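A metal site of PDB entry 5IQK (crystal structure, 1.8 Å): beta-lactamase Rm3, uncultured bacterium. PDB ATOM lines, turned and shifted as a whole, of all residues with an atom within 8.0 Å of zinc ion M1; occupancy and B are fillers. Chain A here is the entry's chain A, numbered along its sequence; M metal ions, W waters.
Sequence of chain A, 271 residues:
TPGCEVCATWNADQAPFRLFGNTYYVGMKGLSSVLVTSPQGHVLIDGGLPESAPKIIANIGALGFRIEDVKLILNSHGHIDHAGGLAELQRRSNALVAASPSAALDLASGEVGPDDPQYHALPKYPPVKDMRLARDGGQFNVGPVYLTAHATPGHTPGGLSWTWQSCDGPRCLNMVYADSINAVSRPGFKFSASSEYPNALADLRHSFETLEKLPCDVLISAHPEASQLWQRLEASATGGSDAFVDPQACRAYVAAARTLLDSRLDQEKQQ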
ATOM      1  N   TRP A  10      -1.653  -5.539  -0.548  1.00  0.00           N
ATOM      2  CA  TRP A  10      -2.360  -4.831   0.515  1.00  0.00           C
ATOM      3  C   TRP A  10      -3.233  -5.767   1.361  1.00  0.00           C
ATOM      4  O   TRP A  10      -3.364  -5.576   2.572  1.00  0.00           O
ATOM      5  CB  TRP A  10      -3.222  -3.717  -0.060  1.00  0.00           C
ATOM      6  CG  TRP A  10      -2.424  -2.507  -0.541  1.00  0.00           C
ATOM      7  CD1 TRP A  10      -1.065  -2.336  -0.482  1.00  0.00           C
ATOM      8  CD2 TRP A  10      -2.950  -1.334  -1.160  1.00  0.00           C
ATOM      9  NE1 TRP A  10      -0.717  -1.103  -1.026  1.00  0.00           N
ATOM     10  CE2 TRP A  10      -1.862  -0.474  -1.439  1.00  0.00           C
ATOM     11  CE3 TRP A  10      -4.235  -0.914  -1.521  1.00  0.00           C
ATOM     12  CZ2 TRP A  10      -2.028   0.773  -2.051  1.00  0.00           C
ATOM     13  CZ3 TRP A  10      -4.396   0.320  -2.127  1.00  0.00           C
ATOM     14  CH2 TRP A  10      -3.299   1.147  -2.378  1.00  0.00           C
ATOM     15  N   LEU A  31      -3.342  -2.883   4.860  1.00  0.00           N
ATOM     16  CA  LEU A  31      -4.554  -2.129   5.161  1.00  0.00           C
ATOM     17  C   LEU A  31      -4.977  -2.352   6.612  1.00  0.00           C
ATOM     18  O   LEU A  31      -5.193  -3.500   7.010  1.00  0.00           O
ATOM     19  CB  LEU A  31      -5.696  -2.564   4.234  1.00  0.00           C
ATOM     20  CG  LEU A  31      -5.468  -2.385   2.736  1.00  0.00           C
ATOM     21  CD1 LEU A  31      -6.548  -3.117   1.956  1.00  0.00           C
ATOM     22  CD2 LEU A  31      -5.450  -0.904   2.396  1.00  0.00           C
ATOM     23  N   SER A  76     -12.443   5.735   7.957  1.00  0.00           N
ATOM     24  CA  SER A  76     -11.444   6.781   7.811  1.00  0.00           C
ATOM     25  C   SER A  76     -11.757   7.605   6.549  1.00  0.00           C
ATOM     26  O   SER A  76     -12.034   8.797   6.631  1.00  0.00           O
ATOM     27  CB  SER A  76     -10.045   6.184   7.733  1.00  0.00           C
ATOM     28  OG  SER A  76      -9.972   5.223   6.693  1.00  0.00           O
ATOM     29  N   HIS A  77     -11.715   6.961   5.384  1.00  0.00           N
ATOM     30  CA  HIS A  77     -12.173   7.642   4.162  1.00  0.00           C
ATOM     31  C   HIS A  77     -12.780   6.663   3.148  1.00  0.00           C
ATOM     32  O   HIS A  77     -12.688   5.448   3.307  1.00  0.00           O
ATOM     33  CB  HIS A  77     -11.053   8.477   3.527  1.00  0.00           C
ATOM     34  CG  HIS A  77      -9.887   7.692   2.966  1.00  0.00           C
ATOM     35  ND1 HIS A  77      -8.876   7.192   3.762  1.00  0.00           N
ATOM     36  CD2 HIS A  77      -9.528   7.418   1.685  1.00  0.00           C
ATOM     37  CE1 HIS A  77      -7.968   6.599   3.001  1.00  0.00           C
ATOM     38  NE2 HIS A  77      -8.341   6.719   1.743  1.00  0.00           N
ATOM     39  N   GLY A  78     -13.370   7.226   2.089  1.00  0.00           N
ATOM     40  CA  GLY A  78     -14.264   6.485   1.219  1.00  0.00           C
ATOM     41  C   GLY A  78     -13.659   5.670   0.091  1.00  0.00           C
ATOM     42  O   GLY A  78     -14.371   5.120  -0.740  1.00  0.00           O
ATOM     43  N   HIS A  79     -12.331   5.619   0.020  1.00  0.00           N
ATOM     44  CA  HIS A  79     -11.707   4.773  -0.990  1.00  0.00           C
ATOM     45  C   HIS A  79     -12.000   3.304  -0.759  1.00  0.00           C
ATOM     46  O   HIS A  79     -12.150   2.884   0.391  1.00  0.00           O
ATOM     47  CB  HIS A  79     -10.203   4.999  -1.025  1.00  0.00           C
ATOM     48  CG  HIS A  79      -9.790   6.262  -1.708  1.00  0.00           C
ATOM     49  ND1 HIS A  79      -8.600   6.884  -1.434  1.00  0.00           N
ATOM     50  CD2 HIS A  79     -10.405   7.013  -2.665  1.00  0.00           C
ATOM     51  CE1 HIS A  79      -8.475   7.963  -2.200  1.00  0.00           C
ATOM     52  NE2 HIS A  79      -9.559   8.068  -2.943  1.00  0.00           N
ATOM     53  N   ILE A  80     -12.051   2.558  -1.852  1.00  0.00           N
ATOM     54  CA  ILE A  80     -12.403   1.143  -1.808  1.00  0.00           C
ATOM     55  C   ILE A  80     -11.522   0.301  -0.879  1.00  0.00           C
ATOM     56  O   ILE A  80     -11.986  -0.711  -0.341  1.00  0.00           O
ATOM     57  CB  ILE A  80     -12.377   0.535  -3.255  1.00  0.00           C
ATOM     58  CG1 ILE A  80     -12.897  -0.908  -3.259  1.00  0.00           C
ATOM     59  CG2 ILE A  80     -10.971   0.619  -3.859  1.00  0.00           C
ATOM     60  CD1 ILE A  80     -13.273  -1.417  -4.654  1.00  0.00           C
ATOM     61  N   ASP A  81     -10.275   0.697  -0.669  1.00  0.00           N
ATOM     62  CA  ASP A  81      -9.391  -0.121   0.160  1.00  0.00           C
ATOM     63  C   ASP A  81      -9.589   0.109   1.656  1.00  0.00           C
ATOM     64  O   ASP A  81      -8.884  -0.517   2.464  1.00  0.00           O
ATOM     65  CB  ASP A  81      -7.910   0.109  -0.206  1.00  0.00           C
ATOM     66  CG  ASP A  81      -7.500   1.576  -0.125  1.00  0.00           C
ATOM     67  OD1 ASP A  81      -8.301   2.422  -0.562  1.00  0.00           O
ATOM     68  OD2 ASP A  81      -6.379   1.880   0.360  1.00  0.00           O
ATOM     69  N   HIS A  82     -10.529   0.990   2.034  1.00  0.00           N
ATOM     70  CA  HIS A  82     -10.893   1.182   3.453  1.00  0.00           C
ATOM     71  C   HIS A  82     -12.397   0.963   3.658  1.00  0.00           C
ATOM     72  O   HIS A  82     -12.851   0.570   4.738  1.00  0.00           O
ATOM     73  CB  HIS A  82     -10.456   2.581   3.923  1.00  0.00           C
ATOM     74  CG  HIS A  82      -9.002   2.853   3.677  1.00  0.00           C
ATOM     75  ND1 HIS A  82      -8.013   2.432   4.544  1.00  0.00           N
ATOM     76  CD2 HIS A  82      -8.365   3.417   2.626  1.00  0.00           C
ATOM     77  CE1 HIS A  82      -6.830   2.757   4.052  1.00  0.00           C
ATOM     78  NE2 HIS A  82      -7.015   3.361   2.886  1.00  0.00           N
ATOM     79  N   ASP A 116     -12.785  13.641  -5.778  1.00  0.00           N
ATOM     80  CA  ASP A 116     -11.792  12.711  -5.268  1.00  0.00           C
ATOM     81  C   ASP A 116     -10.568  12.694  -6.179  1.00  0.00           C
ATOM     82  O   ASP A 116     -10.709  12.652  -7.412  1.00  0.00           O
ATOM     83  CB  ASP A 116     -12.380  11.312  -5.130  1.00  0.00           C
ATOM     84  CG  ASP A 116     -11.545  10.416  -4.228  1.00  0.00           C
ATOM     85  OD1 ASP A 116     -11.990  10.165  -3.090  1.00  0.00           O
ATOM     86  OD2 ASP A 116     -10.462   9.949  -4.659  1.00  0.00           O
ATOM     87  N   GLN A 118      -8.847  10.349  -6.862  1.00  0.00           N
ATOM     88  CA  GLN A 118      -8.863   9.104  -7.629  1.00  0.00           C
ATOM     89  C   GLN A 118     -10.221   8.778  -8.262  1.00  0.00           C
ATOM     90  O   GLN A 118     -10.502   7.629  -8.610  1.00  0.00           O
ATOM     91  CB  GLN A 118      -8.380   7.960  -6.753  1.00  0.00           C
ATOM     92  CG  GLN A 118      -6.973   8.217  -6.230  1.00  0.00           C
ATOM     93  CD  GLN A 118      -6.418   7.083  -5.391  1.00  0.00           C
ATOM     94  OE1 GLN A 118      -5.961   7.304  -4.268  1.00  0.00           O
ATOM     95  NE2 GLN A 118      -6.437   5.873  -5.942  1.00  0.00           N
ATOM     96  N   LEU A 122     -10.895   4.145  -9.697  1.00  0.00           N
ATOM     97  CA  LEU A 122     -11.087   3.054  -8.727  1.00  0.00           C
ATOM     98  C   LEU A 122     -12.367   2.293  -9.058  1.00  0.00           C
ATOM     99  O   LEU A 122     -13.315   2.860  -9.598  1.00  0.00           O
ATOM    100  CB  LEU A 122     -11.125   3.601  -7.298  1.00  0.00           C
ATOM    101  CG  LEU A 122      -9.807   4.119  -6.695  1.00  0.00           C
ATOM    102  CD1 LEU A 122     -10.020   4.787  -5.343  1.00  0.00           C
ATOM    103  CD2 LEU A 122      -8.767   3.023  -6.597  1.00  0.00           C
ATOM    104  N   HIS A 155      -6.058  13.863   1.348  1.00  0.00           N
ATOM    105  CA  HIS A 155      -5.927  12.672   0.520  1.00  0.00           C
ATOM    106  C   HIS A 155      -7.281  12.400  -0.142  1.00  0.00           C
ATOM    107  O   HIS A 155      -7.333  11.941  -1.286  1.00  0.00           O
ATOM    108  CB  HIS A 155      -5.442  11.492   1.369  1.00  0.00           C
ATOM    109  CG  HIS A 155      -5.522  10.160   0.703  1.00  0.00           C
ATOM    110  ND1 HIS A 155      -4.535   9.677  -0.137  1.00  0.00           N
ATOM    111  CD2 HIS A 155      -6.454   9.175   0.780  1.00  0.00           C
ATOM    112  CE1 HIS A 155      -4.862   8.476  -0.566  1.00  0.00           C
ATOM    113  NE2 HIS A 155      -6.019   8.133  -0.004  1.00  0.00           N
ATOM    114  N   THR A 156      -8.359  12.679   0.587  1.00  0.00           N
ATOM    115  CA  THR A 156      -9.725  12.775   0.035  1.00  0.00           C
ATOM    116  C   THR A 156     -10.416  13.939   0.742  1.00  0.00           C
ATOM    117  O   THR A 156      -9.962  14.362   1.807  1.00  0.00           O
ATOM    118  CB  THR A 156     -10.559  11.495   0.249  1.00  0.00           C
ATOM    119  OG1 THR A 156     -10.825  11.326   1.651  1.00  0.00           O
ATOM    120  CG2 THR A 156      -9.852  10.261  -0.291  1.00  0.00           C
ATOM    121  N   ASP A 179      -5.883   8.831   9.517  1.00  0.00           N
ATOM    122  CA  ASP A 179      -6.225   8.600   8.134  1.00  0.00           C
ATOM    123  C   ASP A 179      -5.013   8.856   7.243  1.00  0.00           C
ATOM    124  O   ASP A 179      -4.059   9.534   7.630  1.00  0.00           O
ATOM    125  CB  ASP A 179      -7.385   9.507   7.699  1.00  0.00           C
ATOM    126  CG  ASP A 179      -7.979   9.060   6.375  1.00  0.00           C
ATOM    127  OD1 ASP A 179      -7.757   7.880   5.987  1.00  0.00           O
ATOM    128  OD2 ASP A 179      -8.643   9.880   5.717  1.00  0.00           O
ATOM    129  N   SER A 180      -5.061   8.300   6.042  1.00  0.00           N
ATOM    130  CA  SER A 180      -4.111   8.664   4.988  1.00  0.00           C
ATOM    131  C   SER A 180      -4.092  10.170   4.782  1.00  0.00           C
ATOM    132  O   SER A 180      -5.152  10.779   4.705  1.00  0.00           O
ATOM    133  CB  SER A 180      -4.485   7.998   3.662  1.00  0.00           C
ATOM    134  OG  SER A 180      -4.508   6.584   3.801  1.00  0.00           O
ATOM    135  N   ILE A 181      -2.896  10.749   4.702  1.00  0.00           N
ATOM    136  CA  ILE A 181      -2.728  12.156   4.362  1.00  0.00           C
ATOM    137  C   ILE A 181      -1.669  12.311   3.276  1.00  0.00           C
ATOM    138  O   ILE A 181      -1.033  13.373   3.142  1.00  0.00           O
ATOM    139  CB  ILE A 181      -2.334  12.993   5.593  1.00  0.00           C
ATOM    140  CG1 ILE A 181      -1.165  12.339   6.328  1.00  0.00           C
ATOM    141  CG2 ILE A 181      -3.526  13.141   6.535  1.00  0.00           C
ATOM    142  CD1 ILE A 181      -0.584  13.184   7.433  1.00  0.00           C
ATOM    143  N   ASN A 182      -1.484  11.247   2.488  1.00  0.00           N
ATOM    144  CA  ASN A 182      -0.503  11.298   1.417  1.00  0.00           C
ATOM    145  C   ASN A 182      -1.122  11.850   0.130  1.00  0.00           C
ATOM    146  O   ASN A 182      -2.201  11.435  -0.308  1.00  0.00           O
ATOM    147  CB  ASN A 182       0.123   9.906   1.188  1.00  0.00           C
ATOM    148  CG  ASN A 182      -0.903   8.808   0.854  1.00  0.00           C
ATOM    149  OD1 ASN A 182      -2.034   8.807   1.336  1.00  0.00           O
ATOM    150  ND2 ASN A 182      -0.478   7.844   0.051  1.00  0.00           N
ATOM    151  N   VAL A 184      -1.378  11.559  -3.090  1.00  0.00           N
ATOM    152  CA  VAL A 184      -1.308  10.691  -4.251  1.00  0.00           C
ATOM    153  C   VAL A 184      -2.674  10.734  -4.929  1.00  0.00           C
ATOM    154  O   VAL A 184      -3.688  11.070  -4.293  1.00  0.00           O
ATOM    155  CB  VAL A 184      -0.966   9.242  -3.868  1.00  0.00           C
ATOM    156  CG1 VAL A 184       0.344   9.204  -3.111  1.00  0.00           C
ATOM    157  CG2 VAL A 184      -2.080   8.655  -3.002  1.00  0.00           C
ATOM    158  N   ALA A 222      -3.871   4.318   8.625  1.00  0.00           N
ATOM    159  CA  ALA A 222      -4.792   3.585   7.758  1.00  0.00           C
ATOM    160  C   ALA A 222      -4.042   2.607   6.865  1.00  0.00           C
ATOM    161  O   ALA A 222      -4.502   1.479   6.646  1.00  0.00           O
ATOM    162  CB  ALA A 222      -5.617   4.564   6.930  1.00  0.00           C
ATOM    163  N   HIS A 223      -2.889   3.022   6.360  1.00  0.00           N
ATOM    164  CA  HIS A 223      -1.941   2.082   5.744  1.00  0.00           C
ATOM    165  C   HIS A 223      -0.835   1.831   6.772  1.00  0.00           C
ATOM    166  O   HIS A 223      -0.064   2.749   7.060  1.00  0.00           O
ATOM    167  CB  HIS A 223      -1.378   2.632   4.419  1.00  0.00           C
ATOM    168  CG  HIS A 223      -2.354   2.620   3.288  1.00  0.00           C
ATOM    169  ND1 HIS A 223      -2.287   1.720   2.244  1.00  0.00           N
ATOM    170  CD2 HIS A 223      -3.427   3.417   3.034  1.00  0.00           C
ATOM    171  CE1 HIS A 223      -3.281   1.947   1.406  1.00  0.00           C
ATOM    172  NE2 HIS A 223      -3.980   2.975   1.858  1.00  0.00           N
HETATM  173 ZN    ZN M   1      -7.215   6.473   0.020  1.00  0.00          ZN
HETATM  174 ZN    ZN M   2      -5.831   3.551   1.274  1.00  0.00          ZN
HETATM  175  O   HOH W   1      -5.142   5.823   1.415  1.00  0.00           O
HETATM  176  O   HOH W   2      -6.333   4.826  -0.328  1.00  0.00           O
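Water W2 is bound to zinc ion M1 (1.9 Å).
Zinc ion M1 is bound by a ring nitrogen (NE2) of His 155 (2.0 Å).
A ring nitrogen (ND1) of His 79 binds zinc ion M1, 2.0 Å away.
NE2 of His 77 binds zinc ion M1, at 2.1 Å.
Zinc ion M1 is bound by water W1 (2.6 Å).
Three residues have an atom within 4 Å of zinc ion M1: His 77, His 79 and His 155.
O of Asn 182 sits at hydrogen-bond distance from ND1 of His 155.
A ring nitrogen (NE2) of His 79 is in hydrogen-bond range of the side-chain carboxylate (OD2) of Asp 116.
A ring nitrogen (ND1) of His 77 sits at hydrogen-bond distance from the side-chain carboxylate (OD1) of Asp 179, at 2.6 Å.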
